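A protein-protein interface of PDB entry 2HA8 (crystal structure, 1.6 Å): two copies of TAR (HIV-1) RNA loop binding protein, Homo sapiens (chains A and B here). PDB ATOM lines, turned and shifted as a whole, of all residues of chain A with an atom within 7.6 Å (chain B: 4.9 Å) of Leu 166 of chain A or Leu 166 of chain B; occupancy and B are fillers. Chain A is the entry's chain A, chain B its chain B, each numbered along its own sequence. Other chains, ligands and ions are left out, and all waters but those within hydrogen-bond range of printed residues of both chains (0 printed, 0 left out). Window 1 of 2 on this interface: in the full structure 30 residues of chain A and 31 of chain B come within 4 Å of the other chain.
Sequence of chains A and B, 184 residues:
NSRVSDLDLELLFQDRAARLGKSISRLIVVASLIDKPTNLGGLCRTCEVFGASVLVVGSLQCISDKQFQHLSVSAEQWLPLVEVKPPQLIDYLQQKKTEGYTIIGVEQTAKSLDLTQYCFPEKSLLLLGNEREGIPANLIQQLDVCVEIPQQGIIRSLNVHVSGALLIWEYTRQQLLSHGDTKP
The side-chain carboxylate (OE1) of Glu 170 of chain B lies within hydrogen-bond range of the indole nitrogen (NE1) of Trp 169 of chain A (3.3 Å).
NE2 of His 161 of chain A sits close to OG1 of Thr 46 of chain A. OD1 of Asn 159 of chain A lies within hydrogen-bond range of N of His 161 of chain A. OD1 of Asn 159 of chain A lies within hydrogen-bond range of N of Val 162 of chain A, at 3.1 Å.
Among the printed residues, pairs that only touch across the chains: Trp 169 of chain A with Leu 166 of chain B, Leu 166 of chain A with Trp 169 of chain B, His 161 of chain A with Val 162 of chain B, Trp 169 of chain A with Leu 115 of chain B, Pro 150 of chain A with Phe 50 of chain B, Leu 166 of chain A with Phe 50 of chain B, Leu 115 of chain A with Trp 169 of chain B, Phe 50 of chain A with Leu 166 of chain B, Leu 166 of chain A with Leu 166 of chain B, Ala 165 of chain A with Leu 166 of chain B, Leu 166 of chain A with Ala 165 of chain B, Phe 50 of chain A with Ile 149 of chain B, Ile 149 of chain A with Phe 50 of chain B, Val 49 of chain A with Leu 158 of chain B, Trp 169 of chain A with Trp 169 of chain B, Ala 165 of chain A with Val 162 of chain B, Val 162 of chain A with Ala 165 of chain B, Glu 170 of chain A with Trp 169 of chain B, Leu 158 of chain A with Phe 50 of chain B, Pro 150 of chain A with Trp 169 of chain B and Thr 46 of chain A with Val 162 of chain B.
Of the printed residues of chain B, Pro 150 of chain A touches Phe 50 and Trp 169. Val 160 of chain A touches none of the printed residues of chain B. Printed residues of chain B within 4 Å of His 161 of chain A: Val 162. Of chain B, only Phe 50 (3.6 Å), Ala 165 (3.7 Å), Leu 166 (3.6 Å) and Trp 169 (3.4 Å) come within 4 Å of Leu 166 of chain A. Of the printed residues of chain A, Phe 50 of chain B touches Ile 149 (3.7 Å), Pro 150 (3.5 Å), Leu 158 (3.96 Å) and Leu 166 (3.6 Å). Ala 165 of chain B touches just these residues of chain A: Val 162 (3.9 Å) and Leu 166 (3.7 Å). Of chain A, only Phe 50, Ala 165, Leu 166 and Trp 169 come within 4 Å of Leu 166 of chain B. The nearest printed residue of chain A that does not touch Leu 166 of chain B is Thr 46 of chain A (6.0 Å). The nearest printed residue of chain B that does not touch Val 162 of chain A is Val 162 of chain B (5.1 Å).
Hydrophobic or aromatic side chains of chain A that line the printed part of chain B: Val 49, Phe 50, Leu 115, Ile 149, Pro 150, Leu 158, His 161, Val 162, Ala 165, Leu 166 and Trp 169. Printed residues of chain B that touch a printed residue of chain A: Phe 50, Leu 115, Ile 149, Leu 158, Val 162, Ala 165, Leu 166, Trp 169 and Glu 170. Hydrophobic or aromatic side chains of chain B within 4 Å of the printed part of chain A: Phe 50, Leu 115, Ile 149, Leu 158, Val 162, Ala 165, Leu 166 and Trp 169. Among the printed residues, 22 pairs touch across the chains.
Phe 50 of chain A touches Ile 149 of chain B, and with the chains exchanged Ile 149 of chain A touches Phe 50 of chain B. Phe 50 of chain A touches Leu 166 of chain B, and with the chains exchanged Leu 166 of chain A touches Phe 50 of chain B. Leu 166 of chain A touches its own counterpart, Leu 166 of chain B.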
ATOM      1  N   LEU A  43      15.607 -22.234  30.612  1.00  0.00           N
ATOM      2  CA  LEU A  43      15.312 -22.111  29.192  1.00  0.00           C
ATOM      3  C   LEU A  43      14.268 -23.142  28.757  1.00  0.00           C
ATOM      4  O   LEU A  43      13.396 -22.854  27.927  1.00  0.00           O
ATOM      5  CB  LEU A  43      16.604 -22.267  28.407  1.00  0.00           C
ATOM      6  CG  LEU A  43      16.566 -21.968  26.925  1.00  0.00           C
ATOM      7  CD1 LEU A  43      16.189 -20.505  26.639  1.00  0.00           C
ATOM      8  CD2 LEU A  43      17.951 -22.299  26.402  1.00  0.00           C
ATOM      9  N   THR A  46      10.854 -21.809  29.646  1.00  0.00           N
ATOM     10  CA  THR A  46      10.496 -20.713  28.746  1.00  0.00           C
ATOM     11  C   THR A  46      10.116 -21.214  27.349  1.00  0.00           C
ATOM     12  O   THR A  46       9.116 -20.770  26.764  1.00  0.00           O
ATOM     13  CB  THR A  46      11.638 -19.686  28.667  1.00  0.00           C
ATOM     14  OG1 THR A  46      11.850 -19.155  29.984  1.00  0.00           O
ATOM     15  CG2 THR A  46      11.274 -18.542  27.685  1.00  0.00           C
ATOM     16  N   VAL A  49       6.646 -22.863  27.505  1.00  0.00           N
ATOM     17  CA  VAL A  49       5.613 -21.838  27.618  1.00  0.00           C
ATOM     18  C   VAL A  49       5.299 -21.154  26.290  1.00  0.00           C
ATOM     19  O   VAL A  49       4.123 -20.929  25.962  1.00  0.00           O
ATOM     20  CB  VAL A  49       5.985 -20.789  28.694  1.00  0.00           C
ATOM     21  CG1 VAL A  49       5.076 -19.556  28.576  1.00  0.00           C
ATOM     22  CG2 VAL A  49       5.899 -21.401  30.076  1.00  0.00           C
ATOM     23  N   PHE A  50       6.334 -20.869  25.500  1.00  0.00           N
ATOM     24  CA  PHE A  50       6.144 -20.185  24.230  1.00  0.00           C
ATOM     25  C   PHE A  50       5.985 -21.111  23.034  1.00  0.00           C
ATOM     26  O   PHE A  50       5.951 -20.655  21.885  1.00  0.00           O
ATOM     27  CB  PHE A  50       7.293 -19.198  23.999  1.00  0.00           C
ATOM     28  CG  PHE A  50       7.175 -17.958  24.821  1.00  0.00           C
ATOM     29  CD1 PHE A  50       6.072 -17.105  24.667  1.00  0.00           C
ATOM     30  CD2 PHE A  50       8.139 -17.641  25.759  1.00  0.00           C
ATOM     31  CE1 PHE A  50       5.950 -15.939  25.443  1.00  0.00           C
ATOM     32  CE2 PHE A  50       8.022 -16.475  26.534  1.00  0.00           C
ATOM     33  CZ  PHE A  50       6.927 -15.631  26.372  1.00  0.00           C
ATOM     34  N   LEU A 115      18.129  -6.261  17.609  1.00  0.00           N
ATOM     35  CA  LEU A 115      16.819  -6.915  17.786  1.00  0.00           C
ATOM     36  C   LEU A 115      15.629  -5.991  17.511  1.00  0.00           C
ATOM     37  O   LEU A 115      14.600  -6.443  16.999  1.00  0.00           O
ATOM     38  CB  LEU A 115      16.683  -7.547  19.183  1.00  0.00           C
ATOM     39  CG  LEU A 115      15.406  -8.340  19.490  1.00  0.00           C
ATOM     40  CD1 LEU A 115      15.160  -9.459  18.483  1.00  0.00           C
ATOM     41  CD2 LEU A 115      15.517  -8.934  20.894  1.00  0.00           C
ATOM     42  N   PHE A 120      12.011 -11.544  12.136  1.00  0.00           N
ATOM     43  CA  PHE A 120      12.260 -12.984  12.120  1.00  0.00           C
ATOM     44  C   PHE A 120      11.582 -13.720  10.985  1.00  0.00           C
ATOM     45  O   PHE A 120      10.377 -13.549  10.769  1.00  0.00           O
ATOM     46  CB  PHE A 120      11.791 -13.660  13.402  1.00  0.00           C
ATOM     47  CG  PHE A 120      12.636 -13.348  14.576  1.00  0.00           C
ATOM     48  CD1 PHE A 120      13.710 -14.170  14.898  1.00  0.00           C
ATOM     49  CD2 PHE A 120      12.353 -12.240  15.369  1.00  0.00           C
ATOM     50  CE1 PHE A 120      14.530 -13.877  16.010  1.00  0.00           C
ATOM     51  CE2 PHE A 120      13.156 -11.940  16.491  1.00  0.00           C
ATOM     52  CZ  PHE A 120      14.246 -12.770  16.806  1.00  0.00           C
ATOM     53  N   LEU A 126      17.596 -20.412  16.702  1.00  0.00           N
ATOM     54  CA  LEU A 126      18.364 -19.493  17.561  1.00  0.00           C
ATOM     55  C   LEU A 126      19.532 -20.243  18.164  1.00  0.00           C
ATOM     56  O   LEU A 126      19.321 -21.208  18.888  1.00  0.00           O
ATOM     57  CB  LEU A 126      17.486 -18.950  18.690  1.00  0.00           C
ATOM     58  CG  LEU A 126      16.189 -18.284  18.245  1.00  0.00           C
ATOM     59  CD1 LEU A 126      15.403 -17.786  19.468  1.00  0.00           C
ATOM     60  CD2 LEU A 126      16.462 -17.133  17.284  1.00  0.00           C
ATOM     61  N   ILE A 149      20.797  -7.965  21.357  1.00  0.00           N
ATOM     62  CA  ILE A 149      19.866  -7.164  22.153  1.00  0.00           C
ATOM     63  C   ILE A 149      20.608  -5.899  22.561  1.00  0.00           C
ATOM     64  O   ILE A 149      21.654  -5.999  23.176  1.00  0.00           O
ATOM     65  CB  ILE A 149      19.480  -7.941  23.416  1.00  0.00           C
ATOM     66  CG1 ILE A 149      18.819  -9.287  23.037  1.00  0.00           C
ATOM     67  CG2 ILE A 149      18.547  -7.124  24.286  1.00  0.00           C
ATOM     68  CD1 ILE A 149      18.926 -10.360  24.106  1.00  0.00           C
ATOM     69  N   PRO A 150      20.065  -4.710  22.227  1.00  0.00           N
ATOM     70  CA  PRO A 150      20.782  -3.462  22.612  1.00  0.00           C
ATOM     71  C   PRO A 150      20.776  -3.258  24.132  1.00  0.00           C
ATOM     72  O   PRO A 150      19.768  -3.538  24.786  1.00  0.00           O
ATOM     73  CB  PRO A 150      19.974  -2.355  21.922  1.00  0.00           C
ATOM     74  CG  PRO A 150      18.592  -2.947  21.759  1.00  0.00           C
ATOM     75  CD  PRO A 150      18.812  -4.436  21.503  1.00  0.00           C
ATOM     76  N   LEU A 158      23.732  -9.787  29.105  1.00  0.00           N
ATOM     77  CA  LEU A 158      22.648 -10.431  29.821  1.00  0.00           C
ATOM     78  C   LEU A 158      22.994 -11.888  30.141  1.00  0.00           C
ATOM     79  O   LEU A 158      23.911 -12.460  29.551  1.00  0.00           O
ATOM     80  CB  LEU A 158      21.382 -10.382  28.965  1.00  0.00           C
ATOM     81  CG  LEU A 158      20.784  -8.987  28.738  1.00  0.00           C
ATOM     82  CD1 LEU A 158      19.888  -9.027  27.495  1.00  0.00           C
ATOM     83  CD2 LEU A 158      19.948  -8.571  29.973  1.00  0.00           C
ATOM     84  N   ASN A 159      22.261 -12.479  31.073  1.00  0.00           N
ATOM     85  CA  ASN A 159      22.296 -13.909  31.267  1.00  0.00           C
ATOM     86  C   ASN A 159      21.821 -14.603  29.974  1.00  0.00           C
ATOM     87  O   ASN A 159      20.953 -14.070  29.240  1.00  0.00           O
ATOM     88  CB  ASN A 159      21.409 -14.287  32.454  1.00  0.00           C
ATOM     89  CG  ASN A 159      21.109 -15.759  32.516  1.00  0.00           C
ATOM     90  OD1 ASN A 159      20.114 -16.220  31.943  1.00  0.00           O
ATOM     91  ND2 ASN A 159      21.943 -16.510  33.231  1.00  0.00           N
ATOM     92  N   VAL A 160      22.405 -15.762  29.686  1.00  0.00           N
ATOM     93  CA  VAL A 160      22.117 -16.429  28.394  1.00  0.00           C
ATOM     94  C   VAL A 160      20.645 -16.892  28.267  1.00  0.00           C
ATOM     95  O   VAL A 160      20.059 -16.789  27.179  1.00  0.00           O
ATOM     96  CB  VAL A 160      23.097 -17.590  28.095  1.00  0.00           C
ATOM     97  CG1 VAL A 160      22.918 -18.727  29.087  1.00  0.00           C
ATOM     98  CG2 VAL A 160      22.937 -18.098  26.638  1.00  0.00           C
ATOM     99  N   HIS A 161      20.049 -17.385  29.354  1.00  0.00           N
ATOM    100  CA  HIS A 161      18.622 -17.818  29.317  1.00  0.00           C
ATOM    101  C   HIS A 161      17.732 -16.588  29.110  1.00  0.00           C
ATOM    102  O   HIS A 161      16.809 -16.615  28.307  1.00  0.00           O
ATOM    103  CB  HIS A 161      18.243 -18.575  30.603  1.00  0.00           C
ATOM    104  CG  HIS A 161      16.765 -18.664  30.885  1.00  0.00           C
ATOM    105  ND1 HIS A 161      15.799 -18.691  29.893  1.00  0.00           N
ATOM    106  CD2 HIS A 161      16.095 -18.770  32.059  1.00  0.00           C
ATOM    107  CE1 HIS A 161      14.600 -18.790  30.445  1.00  0.00           C
ATOM    108  NE2 HIS A 161      14.753 -18.862  31.756  1.00  0.00           N
ATOM    109  N   VAL A 162      18.029 -15.498  29.821  1.00  0.00           N
ATOM    110  CA  VAL A 162      17.241 -14.278  29.644  1.00  0.00           C
ATOM    111  C   VAL A 162      17.351 -13.788  28.198  1.00  0.00           C
ATOM    112  O   VAL A 162      16.356 -13.393  27.593  1.00  0.00           O
ATOM    113  CB  VAL A 162      17.674 -13.180  30.638  1.00  0.00           C
ATOM    114  CG1 VAL A 162      17.016 -11.822  30.291  1.00  0.00           C
ATOM    115  CG2 VAL A 162      17.330 -13.621  32.079  1.00  0.00           C
ATOM    116  N   SER A 163      18.561 -13.831  27.636  1.00  0.00           N
ATOM    117  CA  SER A 163      18.790 -13.445  26.227  1.00  0.00           C
ATOM    118  C   SER A 163      17.896 -14.293  25.306  1.00  0.00           C
ATOM    119  O   SER A 163      17.211 -13.763  24.433  1.00  0.00           O
ATOM    120  CB  SER A 163      20.261 -13.652  25.837  1.00  0.00           C
ATOM    121  OG  SER A 163      21.095 -12.800  26.605  1.00  0.00           O
ATOM    122  N   GLY A 164      17.918 -15.604  25.515  1.00  0.00           N
ATOM    123  CA  GLY A 164      17.076 -16.506  24.711  1.00  0.00           C
ATOM    124  C   GLY A 164      15.604 -16.182  24.884  1.00  0.00           C
ATOM    125  O   GLY A 164      14.861 -16.132  23.901  1.00  0.00           O
ATOM    126  N   ALA A 165      15.180 -15.934  26.127  1.00  0.00           N
ATOM    127  CA  ALA A 165      13.767 -15.590  26.382  1.00  0.00           C
ATOM    128  C   ALA A 165      13.365 -14.364  25.597  1.00  0.00           C
ATOM    129  O   ALA A 165      12.263 -14.304  25.047  1.00  0.00           O
ATOM    130  CB  ALA A 165      13.504 -15.362  27.876  1.00  0.00           C
ATOM    131  N   LEU A 166      14.236 -13.349  25.552  1.00  0.00           N
ATOM    132  CA  LEU A 166      13.858 -12.122  24.858  1.00  0.00           C
ATOM    133  C   LEU A 166      13.686 -12.348  23.352  1.00  0.00           C
ATOM    134  O   LEU A 166      12.781 -11.779  22.732  1.00  0.00           O
ATOM    135  CB  LEU A 166      14.882 -11.011  25.134  1.00  0.00           C
ATOM    136  CG  LEU A 166      14.918 -10.495  26.576  1.00  0.00           C
ATOM    137  CD1 LEU A 166      15.844  -9.291  26.601  1.00  0.00           C
ATOM    138  CD2 LEU A 166      13.545 -10.081  27.071  1.00  0.00           C
ATOM    139  N   LEU A 167      14.553 -13.166  22.754  1.00  0.00           N
ATOM    140  CA  LEU A 167      14.391 -13.453  21.312  1.00  0.00           C
ATOM    141  C   LEU A 167      13.194 -14.349  21.042  1.00  0.00           C
ATOM    142  O   LEU A 167      12.509 -14.160  20.046  1.00  0.00           O
ATOM    143  CB  LEU A 167      15.659 -14.039  20.688  1.00  0.00           C
ATOM    144  CG  LEU A 167      16.601 -12.931  20.201  1.00  0.00           C
ATOM    145  CD1 LEU A 167      17.358 -12.322  21.398  1.00  0.00           C
ATOM    146  CD2 LEU A 167      17.561 -13.360  19.122  1.00  0.00           C
ATOM    147  N   ILE A 168      12.956 -15.318  21.923  1.00  0.00           N
ATOM    148  CA  ILE A 168      11.769 -16.185  21.782  1.00  0.00           C
ATOM    149  C   ILE A 168      10.501 -15.327  21.854  1.00  0.00           C
ATOM    150  O   ILE A 168       9.586 -15.491  21.034  1.00  0.00           O
ATOM    151  CB  ILE A 168      11.752 -17.290  22.827  1.00  0.00           C
ATOM    152  CG1 ILE A 168      12.932 -18.266  22.606  1.00  0.00           C
ATOM    153  CG2 ILE A 168      10.396 -18.031  22.829  1.00  0.00           C
ATOM    154  CD1 ILE A 168      13.254 -19.134  23.836  1.00  0.00           C
ATOM    155  N   TRP A 169      10.467 -14.393  22.806  1.00  0.00           N
ATOM    156  CA  TRP A 169       9.346 -13.464  22.919  1.00  0.00           C
ATOM    157  C   TRP A 169       9.196 -12.604  21.669  1.00  0.00           C
ATOM    158  O   TRP A 169       8.095 -12.491  21.129  1.00  0.00           O
ATOM    159  CB  TRP A 169       9.486 -12.550  24.159  1.00  0.00           C
ATOM    160  CG  TRP A 169       8.678 -11.284  24.036  1.00  0.00           C
ATOM    161  CD1 TRP A 169       9.146 -10.035  23.784  1.00  0.00           C
ATOM    162  CD2 TRP A 169       7.253 -11.172  24.092  1.00  0.00           C
ATOM    163  NE1 TRP A 169       8.099  -9.140  23.677  1.00  0.00           N
ATOM    164  CE2 TRP A 169       6.931  -9.819  23.862  1.00  0.00           C
ATOM    165  CE3 TRP A 169       6.219 -12.092  24.291  1.00  0.00           C
ATOM    166  CZ2 TRP A 169       5.610  -9.352  23.852  1.00  0.00           C
ATOM    167  CZ3 TRP A 169       4.893 -11.617  24.288  1.00  0.00           C
ATOM    168  CH2 TRP A 169       4.621 -10.273  24.058  1.00  0.00           C
ATOM    169  N   GLU A 170      10.283 -11.998  21.190  1.00  0.00           N
ATOM    170  CA  GLU A 170      10.171 -11.106  20.038  1.00  0.00           C
ATOM    171  C   GLU A 170       9.705 -11.865  18.789  1.00  0.00           C
ATOM    172  O   GLU A 170       8.859 -11.379  18.057  1.00  0.00           O
ATOM    173  CB  GLU A 170      11.467 -10.321  19.771  1.00  0.00           C
ATOM    174  CG  GLU A 170      11.377  -9.346  18.611  1.00  0.00           C
ATOM    175  CD  GLU A 170      10.391  -8.203  18.811  1.00  0.00           C
ATOM    176  OE1 GLU A 170       9.947  -7.935  19.966  1.00  0.00           O
ATOM    177  OE2 GLU A 170      10.062  -7.576  17.796  1.00  0.00           O
ATOM    178  N   TYR A 171      10.223 -13.075  18.605  1.00  0.00           N
ATOM    179  CA  TYR A 171       9.783 -13.978  17.532  1.00  0.00           C
ATOM    180  C   TYR A 171       8.282 -14.216  17.665  1.00  0.00           C
ATOM    181  O   TYR A 171       7.526 -14.033  16.692  1.00  0.00           O
ATOM    182  CB  TYR A 171      10.536 -15.309  17.601  1.00  0.00           C
ATOM    183  CG  TYR A 171       9.993 -16.342  16.646  1.00  0.00           C
ATOM    184  CD1 TYR A 171      10.497 -16.444  15.341  1.00  0.00           C
ATOM    185  CD2 TYR A 171       8.982 -17.217  17.050  1.00  0.00           C
ATOM    186  CE1 TYR A 171       9.983 -17.403  14.445  1.00  0.00           C
ATOM    187  CE2 TYR A 171       8.454 -18.165  16.172  1.00  0.00           C
ATOM    188  CZ  TYR A 171       8.962 -18.247  14.881  1.00  0.00           C
ATOM    189  OH  TYR A 171       8.432 -19.209  14.036  1.00  0.00           O
ATOM    190  N   THR A 172       7.860 -14.563  18.882  1.00  0.00           N
ATOM    191  CA  THR A 172       6.454 -14.878  19.154  1.00  0.00           C
ATOM    192  C   THR A 172       5.542 -13.668  18.901  1.00  0.00           C
ATOM    193  O   THR A 172       4.511 -13.794  18.239  1.00  0.00           O
ATOM    194  CB  THR A 172       6.279 -15.377  20.583  1.00  0.00           C
ATOM    195  OG1 THR A 172       7.062 -16.563  20.758  1.00  0.00           O
ATOM    196  CG2 THR A 172       4.798 -15.678  20.872  1.00  0.00           C
ATOM    197  N   PHE B  50      19.196  -2.821  31.039  1.00  0.00           N
ATOM    198  CA  PHE B  50      18.191  -2.029  30.318  1.00  0.00           C
ATOM    199  C   PHE B  50      17.963  -0.614  30.845  1.00  0.00           C
ATOM    200  O   PHE B  50      17.076   0.103  30.371  1.00  0.00           O
ATOM    201  CB  PHE B  50      16.860  -2.806  30.216  1.00  0.00           C
ATOM    202  CG  PHE B  50      16.940  -3.968  29.285  1.00  0.00           C
ATOM    203  CD1 PHE B  50      17.316  -3.768  27.945  1.00  0.00           C
ATOM    204  CD2 PHE B  50      16.725  -5.254  29.738  1.00  0.00           C
ATOM    205  CE1 PHE B  50      17.420  -4.858  27.068  1.00  0.00           C
ATOM    206  CE2 PHE B  50      16.808  -6.335  28.870  1.00  0.00           C
ATOM    207  CZ  PHE B  50      17.175  -6.136  27.543  1.00  0.00           C
ATOM    208  N   LEU B 115       0.230  -8.537  26.684  1.00  0.00           N
ATOM    209  CA  LEU B 115       1.442  -7.761  26.431  1.00  0.00           C
ATOM    210  C   LEU B 115       1.618  -7.418  24.953  1.00  0.00           C
ATOM    211  O   LEU B 115       2.156  -6.347  24.616  1.00  0.00           O
ATOM    212  CB  LEU B 115       2.683  -8.518  26.929  1.00  0.00           C
ATOM    213  CG  LEU B 115       4.033  -7.792  26.747  1.00  0.00           C
ATOM    214  CD1 LEU B 115       4.073  -6.420  27.455  1.00  0.00           C
ATOM    215  CD2 LEU B 115       5.129  -8.691  27.281  1.00  0.00           C
ATOM    216  N   ILE B 149       1.511 -11.959  29.968  1.00  0.00           N
ATOM    217  CA  ILE B 149       2.237 -12.514  28.829  1.00  0.00           C
ATOM    218  C   ILE B 149       1.445 -13.737  28.347  1.00  0.00           C
ATOM    219  O   ILE B 149       1.170 -14.640  29.130  1.00  0.00           O
ATOM    220  CB  ILE B 149       3.664 -12.948  29.252  1.00  0.00           C
ATOM    221  CG1 ILE B 149       4.444 -11.745  29.812  1.00  0.00           C
ATOM    222  CG2 ILE B 149       4.446 -13.527  28.069  1.00  0.00           C
ATOM    223  CD1 ILE B 149       5.575 -12.126  30.753  1.00  0.00           C
ATOM    224  N   LEU B 158       5.385 -18.436  33.667  1.00  0.00           N
ATOM    225  CA  LEU B 158       6.837 -18.214  33.539  1.00  0.00           C
ATOM    226  C   LEU B 158       7.482 -17.987  34.916  1.00  0.00           C
ATOM    227  O   LEU B 158       6.789 -17.730  35.903  1.00  0.00           O
ATOM    228  CB  LEU B 158       7.066 -16.994  32.642  1.00  0.00           C
ATOM    229  CG  LEU B 158       6.662 -17.219  31.181  1.00  0.00           C
ATOM    230  CD1 LEU B 158       6.374 -15.879  30.524  1.00  0.00           C
ATOM    231  CD2 LEU B 158       7.805 -17.984  30.481  1.00  0.00           C
ATOM    232  N   VAL B 162      12.060 -13.925  34.565  1.00  0.00           N
ATOM    233  CA  VAL B 162      11.865 -13.949  33.117  1.00  0.00           C
ATOM    234  C   VAL B 162      10.684 -13.062  32.718  1.00  0.00           C
ATOM    235  O   VAL B 162      10.775 -12.280  31.765  1.00  0.00           O
ATOM    236  CB  VAL B 162      11.698 -15.375  32.586  1.00  0.00           C
ATOM    237  CG1 VAL B 162      11.385 -15.350  31.068  1.00  0.00           C
ATOM    238  CG2 VAL B 162      12.966 -16.163  32.886  1.00  0.00           C
ATOM    239  N   SER B 163       9.585 -13.176  33.463  1.00  0.00           N
ATOM    240  CA  SER B 163       8.417 -12.326  33.240  1.00  0.00           C
ATOM    241  C   SER B 163       8.775 -10.845  33.293  1.00  0.00           C
ATOM    242  O   SER B 163       8.418 -10.066  32.384  1.00  0.00           O
ATOM    243  CB  SER B 163       7.324 -12.634  34.290  1.00  0.00           C
ATOM    244  OG  SER B 163       6.874 -13.978  34.138  1.00  0.00           O
ATOM    245  N   GLY B 164       9.489 -10.459  34.353  1.00  0.00           N
ATOM    246  CA  GLY B 164       9.906  -9.057  34.488  1.00  0.00           C
ATOM    247  C   GLY B 164      10.802  -8.656  33.313  1.00  0.00           C
ATOM    248  O   GLY B 164      10.598  -7.623  32.711  1.00  0.00           O
ATOM    249  N   ALA B 165      11.767  -9.506  32.958  1.00  0.00           N
ATOM    250  CA  ALA B 165      12.647  -9.240  31.793  1.00  0.00           C
ATOM    251  C   ALA B 165      11.855  -8.955  30.520  1.00  0.00           C
ATOM    252  O   ALA B 165      12.160  -8.030  29.756  1.00  0.00           O
ATOM    253  CB  ALA B 165      13.628 -10.397  31.549  1.00  0.00           C
ATOM    254  N   LEU B 166      10.824  -9.764  30.276  1.00  0.00           N
ATOM    255  CA  LEU B 166      10.069  -9.582  29.058  1.00  0.00           C
ATOM    256  C   LEU B 166       9.356  -8.226  29.042  1.00  0.00           C
ATOM    257  O   LEU B 166       9.330  -7.553  28.011  1.00  0.00           O
ATOM    258  CB  LEU B 166       9.063 -10.730  28.869  1.00  0.00           C
ATOM    259  CG  LEU B 166       9.702 -12.084  28.515  1.00  0.00           C
ATOM    260  CD1 LEU B 166       8.630 -13.170  28.388  1.00  0.00           C
ATOM    261  CD2 LEU B 166      10.473 -12.001  27.237  1.00  0.00           C
ATOM    262  N   LEU B 167       8.755  -7.832  30.164  1.00  0.00           N
ATOM    263  CA  LEU B 167       8.102  -6.508  30.189  1.00  0.00           C
ATOM    264  C   LEU B 167       9.111  -5.355  30.166  1.00  0.00           C
ATOM    265  O   LEU B 167       8.882  -4.326  29.517  1.00  0.00           O
ATOM    266  CB  LEU B 167       7.152  -6.366  31.381  1.00  0.00           C
ATOM    267  CG  LEU B 167       5.761  -6.901  31.034  1.00  0.00           C
ATOM    268  CD1 LEU B 167       5.769  -8.425  31.111  1.00  0.00           C
ATOM    269  CD2 LEU B 167       4.720  -6.295  31.908  1.00  0.00           C
ATOM    270  N   ILE B 168      10.243  -5.551  30.833  1.00  0.00           N
ATOM    271  CA  ILE B 168      11.290  -4.528  30.811  1.00  0.00           C
ATOM    272  C   ILE B 168      11.772  -4.341  29.369  1.00  0.00           C
ATOM    273  O   ILE B 168      11.895  -3.219  28.872  1.00  0.00           O
ATOM    274  CB  ILE B 168      12.455  -4.880  31.744  1.00  0.00           C
ATOM    275  CG1 ILE B 168      12.013  -4.808  33.211  1.00  0.00           C
ATOM    276  CG2 ILE B 168      13.623  -3.923  31.500  1.00  0.00           C
ATOM    277  CD1 ILE B 168      12.921  -5.578  34.163  1.00  0.00           C
ATOM    278  N   TRP B 169      11.992  -5.449  28.674  1.00  0.00           N
ATOM    279  CA  TRP B 169      12.403  -5.380  27.277  1.00  0.00           C
ATOM    280  C   TRP B 169      11.338  -4.719  26.400  1.00  0.00           C
ATOM    281  O   TRP B 169      11.637  -3.851  25.584  1.00  0.00           O
ATOM    282  CB  TRP B 169      12.793  -6.775  26.772  1.00  0.00           C
ATOM    283  CG  TRP B 169      12.715  -6.849  25.298  1.00  0.00           C
ATOM    284  CD1 TRP B 169      11.767  -7.502  24.567  1.00  0.00           C
ATOM    285  CD2 TRP B 169      13.560  -6.172  24.354  1.00  0.00           C
ATOM    286  NE1 TRP B 169      11.982  -7.300  23.222  1.00  0.00           N
ATOM    287  CE2 TRP B 169      13.078  -6.495  23.066  1.00  0.00           C
ATOM    288  CE3 TRP B 169      14.686  -5.351  24.475  1.00  0.00           C
ATOM    289  CZ2 TRP B 169      13.676  -6.011  21.894  1.00  0.00           C
ATOM    290  CZ3 TRP B 169      15.288  -4.861  23.288  1.00  0.00           C
ATOM    291  CH2 TRP B 169      14.775  -5.201  22.033  1.00  0.00           C
ATOM    292  N   GLU B 170      10.085  -5.140  26.553  1.00  0.00           N
ATOM    293  CA  GLU B 170       9.028  -4.609  25.715  1.00  0.00           C
ATOM    294  C   GLU B 170       8.864  -3.096  25.932  1.00  0.00           C
ATOM    295  O   GLU B 170       8.712  -2.323  24.965  1.00  0.00           O
ATOM    296  CB  GLU B 170       7.739  -5.394  25.943  1.00  0.00           C
ATOM    297  CG  GLU B 170       6.623  -5.077  25.010  1.00  0.00           C
ATOM    298  CD  GLU B 170       6.933  -5.193  23.521  1.00  0.00           C
ATOM    299  OE1 GLU B 170       7.877  -5.914  23.093  1.00  0.00           O
ATOM    300  OE2 GLU B 170       6.187  -4.538  22.778  1.00  0.00           O
